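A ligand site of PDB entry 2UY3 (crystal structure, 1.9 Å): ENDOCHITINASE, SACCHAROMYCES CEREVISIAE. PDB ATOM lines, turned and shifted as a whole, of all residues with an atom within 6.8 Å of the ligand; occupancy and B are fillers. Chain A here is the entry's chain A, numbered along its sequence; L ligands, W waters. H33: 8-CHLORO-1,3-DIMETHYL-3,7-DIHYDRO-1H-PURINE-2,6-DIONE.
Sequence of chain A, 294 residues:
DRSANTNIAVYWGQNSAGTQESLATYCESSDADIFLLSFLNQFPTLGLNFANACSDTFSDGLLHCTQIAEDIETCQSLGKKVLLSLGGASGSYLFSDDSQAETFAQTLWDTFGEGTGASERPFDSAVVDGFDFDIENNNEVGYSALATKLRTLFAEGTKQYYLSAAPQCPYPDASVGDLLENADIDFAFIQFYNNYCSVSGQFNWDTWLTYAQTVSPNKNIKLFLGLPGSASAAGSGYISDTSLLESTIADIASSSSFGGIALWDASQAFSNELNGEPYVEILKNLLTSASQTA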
ATOM      1  N   TYR A  11      33.852  25.280 -24.517  1.00  0.00           N
ATOM      2  CA  TYR A  11      33.060  26.309 -25.167  1.00  0.00           C
ATOM      3  C   TYR A  11      33.970  27.084 -26.116  1.00  0.00           C
ATOM      4  O   TYR A  11      35.106  27.334 -25.799  1.00  0.00           O
ATOM      5  CB  TYR A  11      32.428  27.257 -24.127  1.00  0.00           C
ATOM      6  CG  TYR A  11      31.289  26.577 -23.466  1.00  0.00           C
ATOM      7  CD1 TYR A  11      31.492  25.723 -22.365  1.00  0.00           C
ATOM      8  CD2 TYR A  11      29.976  26.735 -23.960  1.00  0.00           C
ATOM      9  CE1 TYR A  11      30.401  25.030 -21.769  1.00  0.00           C
ATOM     10  CE2 TYR A  11      28.897  26.056 -23.389  1.00  0.00           C
ATOM     11  CZ  TYR A  11      29.118  25.215 -22.289  1.00  0.00           C
ATOM     12  OH  TYR A  11      28.054  24.543 -21.736  1.00  0.00           O
ATOM     13  N   GLN A  14      32.942  33.052 -27.722  1.00  0.00           N
ATOM     14  CA  GLN A  14      32.814  34.323 -27.040  1.00  0.00           C
ATOM     15  C   GLN A  14      34.120  35.006 -26.720  1.00  0.00           C
ATOM     16  O   GLN A  14      34.132  36.029 -26.053  1.00  0.00           O
ATOM     17  CB  GLN A  14      31.947  34.172 -25.796  1.00  0.00           C
ATOM     18  CG  GLN A  14      30.519  33.790 -26.183  1.00  0.00           C
ATOM     19  CD  GLN A  14      29.867  34.938 -26.915  1.00  0.00           C
ATOM     20  OE1 GLN A  14      29.774  36.052 -26.392  1.00  0.00           O
ATOM     21  NE2 GLN A  14      29.495  34.707 -28.154  1.00  0.00           N
ATOM     22  N   SER A  16      36.642  34.654 -24.696  1.00  0.00           N
ATOM     23  CA  SER A  16      36.917  35.051 -23.308  1.00  0.00           C
ATOM     24  C   SER A  16      38.340  35.628 -23.093  1.00  0.00           C
ATOM     25  O   SER A  16      38.542  36.632 -22.374  1.00  0.00           O
ATOM     26  CB  SER A  16      36.622  33.866 -22.391  1.00  0.00           C
ATOM     27  OG  SER A  16      36.981  34.176 -21.060  1.00  0.00           O
ATOM     28  N   SER A  38      29.306  29.085 -29.057  1.00  0.00           N
ATOM     29  CA  SER A  38      28.767  30.042 -28.120  1.00  0.00           C
ATOM     30  C   SER A  38      28.635  31.387 -28.804  1.00  0.00           C
ATOM     31  O   SER A  38      29.663  32.069 -28.960  1.00  0.00           O
ATOM     32  CB  SER A  38      29.738  30.198 -26.923  1.00  0.00           C
ATOM     33  OG  SER A  38      29.879  28.971 -26.202  1.00  0.00           O
ATOM     34  N   PHE A  39      27.411  31.856 -29.130  1.00  0.00           N
ATOM     35  CA  PHE A  39      26.118  31.264 -28.778  1.00  0.00           C
ATOM     36  C   PHE A  39      25.045  31.588 -29.831  1.00  0.00           C
ATOM     37  O   PHE A  39      25.117  32.631 -30.497  1.00  0.00           O
ATOM     38  CB  PHE A  39      25.577  31.900 -27.495  1.00  0.00           C
ATOM     39  CG  PHE A  39      26.310  31.535 -26.227  1.00  0.00           C
ATOM     40  CD1 PHE A  39      26.173  30.287 -25.641  1.00  0.00           C
ATOM     41  CD2 PHE A  39      27.082  32.495 -25.581  1.00  0.00           C
ATOM     42  CE1 PHE A  39      26.848  29.980 -24.433  1.00  0.00           C
ATOM     43  CE2 PHE A  39      27.768  32.176 -24.403  1.00  0.00           C
ATOM     44  CZ  PHE A  39      27.628  30.947 -23.828  1.00  0.00           C
ATOM     45  N   SER A  85      25.492  25.946 -28.860  1.00  0.00           N
ATOM     46  CA  SER A  85      25.007  26.258 -27.528  1.00  0.00           C
ATOM     47  C   SER A  85      23.984  27.406 -27.560  1.00  0.00           C
ATOM     48  O   SER A  85      24.276  28.554 -28.036  1.00  0.00           O
ATOM     49  CB  SER A  85      26.193  26.600 -26.546  1.00  0.00           C
ATOM     50  OG  SER A  85      25.639  26.786 -25.221  1.00  0.00           O
ATOM     51  N   GLY A  87      21.832  30.324 -25.666  1.00  0.00           N
ATOM     52  CA  GLY A  87      21.550  31.135 -24.496  1.00  0.00           C
ATOM     53  C   GLY A  87      22.759  31.965 -24.164  1.00  0.00           C
ATOM     54  O   GLY A  87      23.137  32.826 -24.937  1.00  0.00           O
ATOM     55  N   GLY A  88      23.321  31.699 -23.009  1.00  0.00           N
ATOM     56  CA  GLY A  88      24.413  32.471 -22.484  1.00  0.00           C
ATOM     57  C   GLY A  88      23.978  33.343 -21.342  1.00  0.00           C
ATOM     58  O   GLY A  88      22.843  33.708 -21.250  1.00  0.00           O
ATOM     59  N   ALA A  89      24.908  33.639 -20.458  1.00  0.00           N
ATOM     60  CA  ALA A  89      24.806  34.828 -19.646  1.00  0.00           C
ATOM     61  C   ALA A  89      24.512  35.955 -20.593  1.00  0.00           C
ATOM     62  O   ALA A  89      25.092  36.017 -21.619  1.00  0.00           O
ATOM     63  CB  ALA A  89      26.086  35.071 -18.941  1.00  0.00           C
ATOM     64  N   SER A  90      23.555  36.791 -20.285  1.00  0.00           N
ATOM     65  CA  SER A  90      23.215  37.854 -21.209  1.00  0.00           C
ATOM     66  C   SER A  90      22.827  37.274 -22.565  1.00  0.00           C
ATOM     67  O   SER A  90      22.814  36.110 -22.744  1.00  0.00           O
ATOM     68  CB  SER A  90      24.396  38.799 -21.338  1.00  0.00           C
ATOM     69  OG  SER A  90      25.255  38.417 -22.370  1.00  0.00           O
ATOM     70  N   ASP A 132      23.499  22.483 -27.103  1.00  0.00           N
ATOM     71  CA  ASP A 132      23.729  22.680 -25.693  1.00  0.00           C
ATOM     72  C   ASP A 132      22.738  23.718 -25.166  1.00  0.00           C
ATOM     73  O   ASP A 132      22.478  24.744 -25.823  1.00  0.00           O
ATOM     74  CB  ASP A 132      25.151  23.182 -25.477  1.00  0.00           C
ATOM     75  CG  ASP A 132      25.505  23.428 -24.011  1.00  0.00           C
ATOM     76  OD1 ASP A 132      25.290  22.532 -23.195  1.00  0.00           O
ATOM     77  OD2 ASP A 132      26.070  24.523 -23.677  1.00  0.00           O
ATOM     78  N   ASP A 134      22.595  26.320 -22.529  1.00  0.00           N
ATOM     79  CA  ASP A 134      23.274  27.116 -21.521  1.00  0.00           C
ATOM     80  C   ASP A 134      22.336  28.263 -21.139  1.00  0.00           C
ATOM     81  O   ASP A 134      22.631  29.424 -21.349  1.00  0.00           O
ATOM     82  CB  ASP A 134      24.604  27.641 -22.052  1.00  0.00           C
ATOM     83  CG  ASP A 134      25.423  28.336 -20.982  1.00  0.00           C
ATOM     84  OD1 ASP A 134      25.070  28.249 -19.766  1.00  0.00           O
ATOM     85  OD2 ASP A 134      26.380  29.025 -21.364  1.00  0.00           O
ATOM     86  N   GLU A 136      20.679  30.799 -18.763  1.00  0.00           N
ATOM     87  CA  GLU A 136      21.203  31.467 -17.576  1.00  0.00           C
ATOM     88  C   GLU A 136      20.281  32.608 -17.126  1.00  0.00           C
ATOM     89  O   GLU A 136      20.701  33.529 -16.406  1.00  0.00           O
ATOM     90  CB  GLU A 136      22.636  31.962 -17.834  1.00  0.00           C
ATOM     91  CG  GLU A 136      23.559  30.812 -18.374  1.00  0.00           C
ATOM     92  CD  GLU A 136      25.013  30.900 -17.938  1.00  0.00           C
ATOM     93  OE1 GLU A 136      25.446  31.979 -17.510  1.00  0.00           O
ATOM     94  OE2 GLU A 136      25.742  29.884 -18.061  1.00  0.00           O
ATOM     95  N   ALA A 166      23.907  23.070 -19.510  1.00  0.00           N
ATOM     96  CA  ALA A 166      24.994  23.726 -18.764  1.00  0.00           C
ATOM     97  C   ALA A 166      24.526  24.324 -17.429  1.00  0.00           C
ATOM     98  O   ALA A 166      24.641  25.538 -17.234  1.00  0.00           O
ATOM     99  CB  ALA A 166      25.660  24.829 -19.647  1.00  0.00           C
ATOM    100  N   PRO A 167      24.080  23.474 -16.470  1.00  0.00           N
ATOM    101  CA  PRO A 167      23.589  24.020 -15.200  1.00  0.00           C
ATOM    102  C   PRO A 167      24.763  24.594 -14.415  1.00  0.00           C
ATOM    103  O   PRO A 167      25.903  24.250 -14.700  1.00  0.00           O
ATOM    104  CB  PRO A 167      23.059  22.759 -14.456  1.00  0.00           C
ATOM    105  CG  PRO A 167      23.884  21.668 -14.976  1.00  0.00           C
ATOM    106  CD  PRO A 167      24.018  22.001 -16.473  1.00  0.00           C
ATOM    107  N   PHE A 189      27.051  19.593 -18.488  1.00  0.00           N
ATOM    108  CA  PHE A 189      28.270  20.338 -18.264  1.00  0.00           C
ATOM    109  C   PHE A 189      27.998  21.251 -17.081  1.00  0.00           C
ATOM    110  O   PHE A 189      27.494  22.358 -17.247  1.00  0.00           O
ATOM    111  CB  PHE A 189      28.663  21.134 -19.529  1.00  0.00           C
ATOM    112  CG  PHE A 189      28.775  20.279 -20.793  1.00  0.00           C
ATOM    113  CD1 PHE A 189      29.677  19.207 -20.868  1.00  0.00           C
ATOM    114  CD2 PHE A 189      27.977  20.543 -21.917  1.00  0.00           C
ATOM    115  CE1 PHE A 189      29.794  18.448 -22.012  1.00  0.00           C
ATOM    116  CE2 PHE A 189      28.082  19.768 -23.066  1.00  0.00           C
ATOM    117  CZ  PHE A 189      28.998  18.717 -23.120  1.00  0.00           C
ATOM    118  N   GLN A 191      28.655  23.654 -14.122  1.00  0.00           N
ATOM    119  CA  GLN A 191      29.602  24.738 -13.806  1.00  0.00           C
ATOM    120  C   GLN A 191      29.937  24.770 -12.331  1.00  0.00           C
ATOM    121  O   GLN A 191      29.151  25.282 -11.510  1.00  0.00           O
ATOM    122  CB  GLN A 191      29.063  26.100 -14.235  1.00  0.00           C
ATOM    123  CG  GLN A 191      28.454  26.182 -15.615  1.00  0.00           C
ATOM    124  CD  GLN A 191      27.835  27.565 -15.939  1.00  0.00           C
ATOM    125  OE1 GLN A 191      28.333  28.601 -15.513  1.00  0.00           O
ATOM    126  NE2 GLN A 191      26.768  27.568 -16.733  1.00  0.00           N
ATOM    127  N   TYR A 193      31.942  26.603 -10.599  1.00  0.00           N
ATOM    128  CA  TYR A 193      32.649  27.883 -10.438  1.00  0.00           C
ATOM    129  C   TYR A 193      31.595  29.009 -10.370  1.00  0.00           C
ATOM    130  O   TYR A 193      30.433  28.804 -10.737  1.00  0.00           O
ATOM    131  CB  TYR A 193      33.667  28.103 -11.587  1.00  0.00           C
ATOM    132  CG  TYR A 193      33.081  28.003 -12.988  1.00  0.00           C
ATOM    133  CD1 TYR A 193      33.071  26.779 -13.690  1.00  0.00           C
ATOM    134  CD2 TYR A 193      32.538  29.134 -13.619  1.00  0.00           C
ATOM    135  CE1 TYR A 193      32.553  26.682 -14.966  1.00  0.00           C
ATOM    136  CE2 TYR A 193      31.986  29.033 -14.932  1.00  0.00           C
ATOM    137  CZ  TYR A 193      32.009  27.799 -15.593  1.00  0.00           C
ATOM    138  OH  TYR A 193      31.457  27.664 -16.875  1.00  0.00           O
ATOM    139  N   ASN A 194      32.018  30.201  -9.925  1.00  0.00           N
ATOM    140  CA  ASN A 194      31.114  31.328  -9.591  1.00  0.00           C
ATOM    141  C   ASN A 194      30.012  30.970  -8.572  1.00  0.00           C
ATOM    142  O   ASN A 194      28.943  31.608  -8.542  1.00  0.00           O
ATOM    143  CB  ASN A 194      30.455  31.926 -10.846  1.00  0.00           C
ATOM    144  CG  ASN A 194      31.455  32.516 -11.831  1.00  0.00           C
ATOM    145  OD1 ASN A 194      32.509  33.039 -11.460  1.00  0.00           O
ATOM    146  ND2 ASN A 194      31.086  32.458 -13.113  1.00  0.00           N
ATOM    147  N   PRO A 228      36.611  26.826 -14.997  1.00  0.00           N
ATOM    148  CA  PRO A 228      37.205  27.912 -15.795  1.00  0.00           C
ATOM    149  C   PRO A 228      38.519  27.468 -16.407  1.00  0.00           C
ATOM    150  O   PRO A 228      39.273  26.692 -15.771  1.00  0.00           O
ATOM    151  CB  PRO A 228      37.445  29.021 -14.780  1.00  0.00           C
ATOM    152  CG  PRO A 228      36.559  28.673 -13.582  1.00  0.00           C
ATOM    153  CD  PRO A 228      36.599  27.163 -13.562  1.00  0.00           C
ATOM    154  N   ALA A 233      38.906  33.412 -16.117  1.00  0.00           N
ATOM    155  CA  ALA A 233      37.867  32.970 -17.013  1.00  0.00           C
ATOM    156  C   ALA A 233      36.533  33.115 -16.356  1.00  0.00           C
ATOM    157  O   ALA A 233      35.506  33.145 -17.004  1.00  0.00           O
ATOM    158  CB  ALA A 233      38.086  31.583 -17.367  1.00  0.00           C
ATOM    159  N   ALA A 234      36.578  33.169 -15.047  1.00  0.00           N
ATOM    160  CA  ALA A 234      35.404  33.371 -14.200  1.00  0.00           C
ATOM    161  C   ALA A 234      35.897  34.170 -13.010  1.00  0.00           C
ATOM    162  O   ALA A 234      37.105  34.390 -12.866  1.00  0.00           O
ATOM    163  CB  ALA A 234      34.848  32.036 -13.753  1.00  0.00           C
ATOM    164  N   GLY A 235      34.969  34.591 -12.154  1.00  0.00           N
ATOM    165  CA  GLY A 235      35.332  35.340 -10.964  1.00  0.00           C
ATOM    166  C   GLY A 235      36.037  34.454  -9.955  1.00  0.00           C
ATOM    167  O   GLY A 235      36.992  34.922  -9.277  1.00  0.00           O
ATOM    168  N   TRP A 264      35.276  26.626 -19.738  1.00  0.00           N
ATOM    169  CA  TRP A 264      34.969  27.937 -20.259  1.00  0.00           C
ATOM    170  C   TRP A 264      36.239  28.767 -20.331  1.00  0.00           C
ATOM    171  O   TRP A 264      36.748  29.109 -19.300  1.00  0.00           O
ATOM    172  CB  TRP A 264      33.962  28.688 -19.339  1.00  0.00           C
ATOM    173  CG  TRP A 264      33.689  30.051 -19.939  1.00  0.00           C
ATOM    174  CD1 TRP A 264      34.314  31.229 -19.637  1.00  0.00           C
ATOM    175  CD2 TRP A 264      32.779  30.335 -21.009  1.00  0.00           C
ATOM    176  NE1 TRP A 264      33.829  32.250 -20.437  1.00  0.00           N
ATOM    177  CE2 TRP A 264      32.878  31.717 -21.272  1.00  0.00           C
ATOM    178  CE3 TRP A 264      31.859  29.562 -21.734  1.00  0.00           C
ATOM    179  CZ2 TRP A 264      32.083  32.353 -22.241  1.00  0.00           C
ATOM    180  CZ3 TRP A 264      31.076  30.202 -22.707  1.00  0.00           C
ATOM    181  CH2 TRP A 264      31.220  31.577 -22.961  1.00  0.00           C
HETATM  182  N1  H33 L   1      29.595  33.407 -19.714  1.00  0.00           N
HETATM  183  C2  H33 L   1      28.796  32.344 -20.171  1.00  0.00           C
HETATM  184  C3  H33 L   1      29.031  31.034 -19.701  1.00  0.00           C
HETATM  185  C4  H33 L   1      30.043  30.780 -18.781  1.00  0.00           C
HETATM  186  N5  H33 L   1      30.857  31.833 -18.286  1.00  0.00           N
HETATM  187  C6  H33 L   1      30.630  33.153 -18.766  1.00  0.00           C
HETATM  188  N7  H33 L   1      28.441  29.839 -19.941  1.00  0.00           N
HETATM  189  C8  H33 L   1      29.068  28.905 -19.206  1.00  0.00           C
HETATM  190  N9  H33 L   1      30.033  29.467 -18.495  1.00  0.00           N
HETATM  191  C11 H33 L   1      31.931  31.577 -17.294  1.00  0.00           C
HETATM  192  C15 H33 L   1      29.335  34.774 -20.237  1.00  0.00           C
HETATM  193  O19 H33 L   1      31.334  34.084 -18.360  1.00  0.00           O
HETATM  194  O20 H33 L   1      27.906  32.624 -20.996  1.00  0.00           O
HETATM  195 CL   H33 L   1      28.763  27.396 -19.170  1.00  0.00          CL
HETATM  196  O   HOH W   1      28.856  24.395 -18.824  1.00  0.00           O
HETATM  197  O   HOH W   2      29.430  35.818 -23.471  1.00  0.00           O
HETATM  198  O   HOH W   3      29.157  33.895 -16.207  1.00  0.00           O
HETATM  199  O   HOH W   4      31.913  34.862 -15.433  1.00  0.00           O
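Water W1 bridges the backbone carbonyl oxygen of Phe 189 (2.9 Å) and the side-chain hydroxyl of Tyr 11 (3.0 Å).
Water W4 lies within hydrogen-bond range of an oxygen (O19) of the ligand (3.1 Å) and the side-chain amide nitrogen (ND2) of Asn 194 (3.4 Å).
The side-chain carboxylate (OD1) of Asp 134 lies close to the side-chain carboxylate (OE2) of Glu 136, at 2.5 Å.
O of Asp 134 is in hydrogen-bond range of N of Gly 88 (2.9 Å).
NE2 of Gln 191 lies within hydrogen-bond range of OE2 of Glu 136 (2.9 Å).
The side-chain amide nitrogen (NE2) of Gln 191 is in hydrogen-bond range of the backbone carbonyl oxygen (O) of Ala 166 (3.0 Å).
The backbone carbonyl oxygen (O) of Pro 167 lies within hydrogen-bond range of the backbone NH (N) of Gln 191.
The side-chain carboxylate (OE1) of Glu 136 lies within hydrogen-bond range of the backbone NH (N) of Ala 89, 3.4 Å away.
The side-chain carboxylate of Asp 132 sits at hydrogen-bond distance from the side-chain hydroxyl of Tyr 11, 2.8 Å away.
OD2 of Asp 134 is in hydrogen-bond range of N7 of the ligand (2.6 Å).
OH of Tyr 193 sits close to N9 of the ligand.
An oxygen (O20) of the ligand lies within hydrogen-bond range of the backbone NH of Ala 89 (3.2 Å).
OE2 of Glu 136 lies within hydrogen-bond range of N7 of the ligand, at 3.3 Å.
Residues that only touch the ligand: Tyr 11 (3.8 Å), Phe 39 (3.3 Å), Gly 88 (3.8 Å), Gln 191 (3.2 Å), Ala 233 (3.9 Å) and Trp 264 (3.4 Å).
Hydrophobic or aromatic side chains within 4 Å of the ligand: Tyr 11, Phe 39, Ala 89, Tyr 193 and Trp 264.
Of the 24 residues printed, 10 come within 4 Å of the ligand.
The nearest printed residue that does not touch the ligand is Ala 166 (4.1 Å).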
